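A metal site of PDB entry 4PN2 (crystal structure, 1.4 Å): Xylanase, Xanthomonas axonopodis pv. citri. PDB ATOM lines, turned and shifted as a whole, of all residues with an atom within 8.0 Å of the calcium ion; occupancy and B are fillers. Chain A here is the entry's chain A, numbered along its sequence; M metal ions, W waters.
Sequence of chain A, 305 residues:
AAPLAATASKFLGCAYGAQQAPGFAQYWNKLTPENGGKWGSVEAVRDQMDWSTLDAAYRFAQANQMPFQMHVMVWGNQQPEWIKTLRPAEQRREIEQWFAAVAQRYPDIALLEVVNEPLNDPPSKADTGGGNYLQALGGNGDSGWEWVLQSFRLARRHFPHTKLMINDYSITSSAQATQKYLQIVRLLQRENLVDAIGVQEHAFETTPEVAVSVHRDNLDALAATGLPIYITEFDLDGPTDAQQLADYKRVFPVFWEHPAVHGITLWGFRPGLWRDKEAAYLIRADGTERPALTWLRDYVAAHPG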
ATOM      1  N   TRP A  39     -14.343  26.247  15.367  1.00  0.00           N
ATOM      2  CA  TRP A  39     -13.068  25.827  15.963  1.00  0.00           C
ATOM      3  C   TRP A  39     -13.051  24.372  16.367  1.00  0.00           C
ATOM      4  O   TRP A  39     -12.040  23.697  16.197  1.00  0.00           O
ATOM      5  CB  TRP A  39     -12.690  26.792  17.108  1.00  0.00           C
ATOM      6  CG  TRP A  39     -11.304  26.632  17.691  1.00  0.00           C
ATOM      7  CD1 TRP A  39     -10.254  25.900  17.200  1.00  0.00           C
ATOM      8  CD2 TRP A  39     -10.808  27.329  18.845  1.00  0.00           C
ATOM      9  NE1 TRP A  39      -9.110  26.129  17.974  1.00  0.00           N
ATOM     10  CE2 TRP A  39      -9.434  26.955  19.016  1.00  0.00           C
ATOM     11  CE3 TRP A  39     -11.414  28.206  19.788  1.00  0.00           C
ATOM     12  CZ2 TRP A  39      -8.655  27.447  20.061  1.00  0.00           C
ATOM     13  CZ3 TRP A  39     -10.615  28.716  20.822  1.00  0.00           C
ATOM     14  CH2 TRP A  39      -9.256  28.322  20.948  1.00  0.00           C
ATOM     15  N   GLU A  43      -9.971  21.785  15.403  1.00  0.00           N
ATOM     16  CA  GLU A  43      -9.047  21.436  16.471  1.00  0.00           C
ATOM     17  C   GLU A  43      -9.776  20.652  17.544  1.00  0.00           C
ATOM     18  O   GLU A  43      -9.752  20.990  18.759  1.00  0.00           O
ATOM     19  CB  GLU A  43      -8.295  22.665  16.960  1.00  0.00           C
ATOM     20  CG  GLU A  43      -7.016  22.314  17.720  1.00  0.00           C
ATOM     21  CD  GLU A  43      -6.208  23.496  18.173  1.00  0.00           C
ATOM     22  OE1 GLU A  43      -6.538  24.665  17.865  1.00  0.00           O
ATOM     23  OE2 GLU A  43      -5.178  23.263  18.875  1.00  0.00           O
ATOM     24  N   VAL A  45      -8.998  17.810  18.607  1.00  0.00           N
ATOM     25  CA  VAL A  45      -7.858  17.342  19.423  1.00  0.00           C
ATOM     26  C   VAL A  45      -6.790  18.426  19.471  1.00  0.00           C
ATOM     27  O   VAL A  45      -6.409  18.981  18.411  1.00  0.00           O
ATOM     28  CB  VAL A  45      -7.269  16.026  18.859  1.00  0.00           C
ATOM     29  CG1 VAL A  45      -6.112  15.623  19.699  1.00  0.00           C
ATOM     30  CG2 VAL A  45      -8.302  14.906  18.846  1.00  0.00           C
ATOM     31  N   ARG A  46      -6.374  18.761  20.699  1.00  0.00           N
ATOM     32  CA  ARG A  46      -5.442  19.902  20.868  1.00  0.00           C
ATOM     33  C   ARG A  46      -4.166  19.719  20.009  1.00  0.00           C
ATOM     34  O   ARG A  46      -3.478  18.672  20.063  1.00  0.00           O
ATOM     35  CB  ARG A  46      -5.143  20.116  22.346  1.00  0.00           C
ATOM     36  CG  ARG A  46      -4.359  21.353  22.607  1.00  0.00           C
ATOM     37  CD  ARG A  46      -3.832  21.344  24.016  1.00  0.00           C
ATOM     38  NE  ARG A  46      -3.321  22.641  24.431  1.00  0.00           N
ATOM     39  CZ  ARG A  46      -2.946  22.926  25.688  1.00  0.00           C
ATOM     40  NH1 ARG A  46      -2.919  21.908  26.594  1.00  0.00           N
ATOM     41  NH2 ARG A  46      -2.574  24.166  26.015  1.00  0.00           N
ATOM     42  N   ASP A  47      -3.814  20.804  19.294  1.00  0.00           N
ATOM     43  CA  ASP A  47      -2.551  20.893  18.499  1.00  0.00           C
ATOM     44  C   ASP A  47      -2.481  19.903  17.357  1.00  0.00           C
ATOM     45  O   ASP A  47      -1.417  19.608  16.859  1.00  0.00           O
ATOM     46  CB  ASP A  47      -1.267  20.951  19.343  1.00  0.00           C
ATOM     47  CG  ASP A  47      -1.212  22.210  20.216  1.00  0.00           C
ATOM     48  OD1 ASP A  47      -1.957  23.351  20.020  1.00  0.00           O
ATOM     49  OD2 ASP A  47      -0.545  22.003  21.223  1.00  0.00           O
ATOM     50  N   GLN A  48      -3.629  19.454  16.846  1.00  0.00           N
ATOM     51  CA  GLN A  48      -3.610  18.833  15.536  1.00  0.00           C
ATOM     52  C   GLN A  48      -4.794  19.421  14.793  1.00  0.00           C
ATOM     53  O   GLN A  48      -5.905  19.500  15.321  1.00  0.00           O
ATOM     54  CB  GLN A  48      -3.590  17.319  15.565  1.00  0.00           C
ATOM     55  CG  GLN A  48      -4.722  16.663  16.289  1.00  0.00           C
ATOM     56  CD  GLN A  48      -4.572  15.140  16.379  1.00  0.00           C
ATOM     57  OE1 GLN A  48      -3.645  14.579  17.011  1.00  0.00           O
ATOM     58  NE2 GLN A  48      -5.559  14.449  15.757  1.00  0.00           N
ATOM     59  N   MET A  49      -4.506  20.003  13.646  1.00  0.00           N
ATOM     60  CA  MET A  49      -5.522  20.798  12.937  1.00  0.00           C
ATOM     61  C   MET A  49      -6.001  19.928  11.788  1.00  0.00           C
ATOM     62  O   MET A  49      -5.201  19.489  10.954  1.00  0.00           O
ATOM     63  CB  MET A  49      -4.950  22.150  12.409  1.00  0.00           C
ATOM     64  CG  MET A  49      -4.183  23.032  13.451  1.00  0.00           C
ATOM     65  SD  MET A  49      -5.279  23.469  14.809  1.00  0.00           S
ATOM     66  CE  MET A  49      -5.814  25.115  14.323  1.00  0.00           C
ATOM     67  N   TRP A  82     -11.242  20.337  24.794  1.00  0.00           N
ATOM     68  CA  TRP A  82     -10.042  20.321  25.681  1.00  0.00           C
ATOM     69  C   TRP A  82      -9.744  21.726  26.249  1.00  0.00           C
ATOM     70  O   TRP A  82      -8.947  21.848  27.193  1.00  0.00           O
ATOM     71  CB  TRP A  82      -8.807  19.822  24.931  1.00  0.00           C
ATOM     72  CG  TRP A  82      -8.692  20.450  23.592  1.00  0.00           C
ATOM     73  CD1 TRP A  82      -9.126  19.932  22.364  1.00  0.00           C
ATOM     74  CD2 TRP A  82      -8.098  21.718  23.302  1.00  0.00           C
ATOM     75  NE1 TRP A  82      -8.804  20.823  21.352  1.00  0.00           N
ATOM     76  CE2 TRP A  82      -8.208  21.931  21.879  1.00  0.00           C
ATOM     77  CE3 TRP A  82      -7.474  22.710  24.110  1.00  0.00           C
ATOM     78  CZ2 TRP A  82      -7.707  23.116  21.229  1.00  0.00           C
ATOM     79  CZ3 TRP A  82      -6.994  23.900  23.455  1.00  0.00           C
ATOM     80  CH2 TRP A  82      -7.112  24.063  22.031  1.00  0.00           C
ATOM     81  N   GLU A  90      -3.699  30.168  29.368  1.00  0.00           N
ATOM     82  CA  GLU A  90      -3.453  29.146  28.347  1.00  0.00           C
ATOM     83  C   GLU A  90      -4.535  29.089  27.285  1.00  0.00           C
ATOM     84  O   GLU A  90      -4.262  28.908  26.104  1.00  0.00           O
ATOM     85  CB  GLU A  90      -3.217  27.755  28.970  1.00  0.00           C
ATOM     86  CG  GLU A  90      -1.914  27.624  29.803  1.00  0.00           C
ATOM     87  CD  GLU A  90      -0.626  27.946  29.115  1.00  0.00           C
ATOM     88  OE1 GLU A  90      -0.620  27.983  27.872  1.00  0.00           O
ATOM     89  OE2 GLU A  90       0.412  28.117  29.877  1.00  0.00           O
ATOM     90  N   ARG A  93      -3.715  31.866  24.756  1.00  0.00           N
ATOM     91  CA  ARG A  93      -2.691  31.503  23.773  1.00  0.00           C
ATOM     92  C   ARG A  93      -3.228  30.575  22.717  1.00  0.00           C
ATOM     93  O   ARG A  93      -2.848  30.636  21.520  1.00  0.00           O
ATOM     94  CB  ARG A  93      -1.534  30.876  24.481  1.00  0.00           C
ATOM     95  CG  ARG A  93      -0.793  31.824  25.430  1.00  0.00           C
ATOM     96  CD  ARG A  93       0.213  31.064  26.234  1.00  0.00           C
ATOM     97  NE  ARG A  93       1.477  30.826  25.555  1.00  0.00           N
ATOM     98  CZ  ARG A  93       2.353  29.890  25.879  1.00  0.00           C
ATOM     99  NH1 ARG A  93       2.150  28.955  26.777  1.00  0.00           N
ATOM    100  NH2 ARG A  93       3.507  29.877  25.241  1.00  0.00           N
ATOM    101  N   GLU A  94      -4.125  29.677  23.101  1.00  0.00           N
ATOM    102  CA  GLU A  94      -4.787  28.844  22.068  1.00  0.00           C
ATOM    103  C   GLU A  94      -5.680  29.665  21.104  1.00  0.00           C
ATOM    104  O   GLU A  94      -5.767  29.345  19.919  1.00  0.00           O
ATOM    105  CB  GLU A  94      -5.612  27.747  22.786  1.00  0.00           C
ATOM    106  CG  GLU A  94      -4.678  26.778  23.565  1.00  0.00           C
ATOM    107  CD  GLU A  94      -3.941  25.819  22.686  1.00  0.00           C
ATOM    108  OE1 GLU A  94      -4.162  25.823  21.436  1.00  0.00           O
ATOM    109  OE2 GLU A  94      -3.062  25.058  23.224  1.00  0.00           O
ATOM    110  N   ILE A  95      -6.376  30.635  21.636  1.00  0.00           N
ATOM    111  CA  ILE A  95      -7.282  31.473  20.806  1.00  0.00           C
ATOM    112  C   ILE A  95      -6.376  32.218  19.788  1.00  0.00           C
ATOM    113  O   ILE A  95      -6.661  32.206  18.581  1.00  0.00           O
ATOM    114  CB  ILE A  95      -8.166  32.431  21.645  1.00  0.00           C
ATOM    115  CG1 ILE A  95      -9.162  31.626  22.490  1.00  0.00           C
ATOM    116  CG2 ILE A  95      -8.968  33.398  20.739  1.00  0.00           C
ATOM    117  CD1 ILE A  95      -9.693  32.459  23.615  1.00  0.00           C
ATOM    118  N   GLU A  96      -5.314  32.830  20.308  1.00  0.00           N
ATOM    119  CA  GLU A  96      -4.406  33.561  19.455  1.00  0.00           C
ATOM    120  C   GLU A  96      -3.829  32.652  18.352  1.00  0.00           C
ATOM    121  O   GLU A  96      -3.704  33.072  17.202  1.00  0.00           O
ATOM    122  CB  GLU A  96      -3.242  34.222  20.240  1.00  0.00           C
ATOM    123  CG  GLU A  96      -2.573  35.229  19.313  1.00  0.00           C
ATOM    124  CD  GLU A  96      -2.124  36.549  19.982  1.00  0.00           C
ATOM    125  OE1 GLU A  96      -2.041  36.583  21.243  1.00  0.00           O
ATOM    126  OE2 GLU A  96      -1.808  37.556  19.224  1.00  0.00           O
ATOM    127  N   GLN A  97      -3.400  31.434  18.741  1.00  0.00           N
ATOM    128  CA  GLN A  97      -2.847  30.545  17.766  1.00  0.00           C
ATOM    129  C   GLN A  97      -3.877  30.142  16.709  1.00  0.00           C
ATOM    130  O   GLN A  97      -3.579  30.061  15.525  1.00  0.00           O
ATOM    131  CB  GLN A  97      -2.307  29.305  18.451  1.00  0.00           C
ATOM    132  CG  GLN A  97      -1.842  28.234  17.492  1.00  0.00           C
ATOM    133  CD  GLN A  97      -1.025  27.207  18.220  1.00  0.00           C
ATOM    134  OE1 GLN A  97      -1.505  26.535  19.146  1.00  0.00           O
ATOM    135  NE2 GLN A  97       0.216  27.089  17.842  1.00  0.00           N
ATOM    136  N   TRP A  98      -5.120  29.942  17.111  1.00  0.00           N
ATOM    137  CA  TRP A  98      -6.258  29.676  16.157  1.00  0.00           C
ATOM    138  C   TRP A  98      -6.468  30.826  15.158  1.00  0.00           C
ATOM    139  O   TRP A  98      -6.604  30.633  13.911  1.00  0.00           O
ATOM    140  CB  TRP A  98      -7.442  29.341  16.998  1.00  0.00           C
ATOM    141  CG  TRP A  98      -8.853  29.448  16.396  1.00  0.00           C
ATOM    142  CD1 TRP A  98      -9.872  30.212  16.899  1.00  0.00           C
ATOM    143  CD2 TRP A  98      -9.414  28.733  15.242  1.00  0.00           C
ATOM    144  NE1 TRP A  98     -11.020  30.014  16.134  1.00  0.00           N
ATOM    145  CE2 TRP A  98     -10.761  29.147  15.107  1.00  0.00           C
ATOM    146  CE3 TRP A  98      -8.887  27.822  14.299  1.00  0.00           C
ATOM    147  CZ2 TRP A  98     -11.600  28.690  14.054  1.00  0.00           C
ATOM    148  CZ3 TRP A  98      -9.715  27.304  13.281  1.00  0.00           C
ATOM    149  CH2 TRP A  98     -11.037  27.744  13.147  1.00  0.00           C
ATOM    150  N   ALA A 101      -3.425  30.880  12.818  1.00  0.00           N
ATOM    151  CA  ALA A 101      -3.512  29.701  11.898  1.00  0.00           C
ATOM    152  C   ALA A 101      -4.409  29.925  10.696  1.00  0.00           C
ATOM    153  O   ALA A 101      -4.055  29.566   9.534  1.00  0.00           O
ATOM    154  CB  ALA A 101      -3.966  28.432  12.653  1.00  0.00           C
HETATM  155 CA    CA M   1      -3.458  25.007  19.342  1.00  0.00          CA
HETATM  156  O   HOH W   1      -2.869  24.454  16.908  1.00  0.00           O
HETATM  157  O   HOH W   2      -4.901  26.775  18.615  1.00  0.00           O
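OE1 of Glu 43 is in hydrogen-bond range of NE1 of Trp 39. The indole nitrogen of Trp 82 sits at hydrogen-bond distance from the backbone carbonyl oxygen of Glu 43, 2.8 Å away. OE2 of Glu 94 lies within salt-bridge range of NE of Arg 46 (2.7 Å).
Four residues have an atom within 4 Å of the calcium ion: Glu 43, Asp 47, Glu 94 and Gln 97. The nearest printed residue that does not touch the calcium ion is Trp 82 (4.6 Å).
The calcium ion is bound by the side-chain carboxylate of Asp 47 (2.3 Å), the side-chain carboxylate of Glu 94 (2.4 Å), water W2 (2.4 Å), the side-chain amide oxygen of Gln 97 (2.5 Å), the side-chain carboxylate of Glu 43 (2.5 Å) and water W1 (2.6 Å).
Water W2 lies within hydrogen-bond range of OE1 of Glu 43 (2.8 Å) and O of Glu 94 (3.0 Å).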
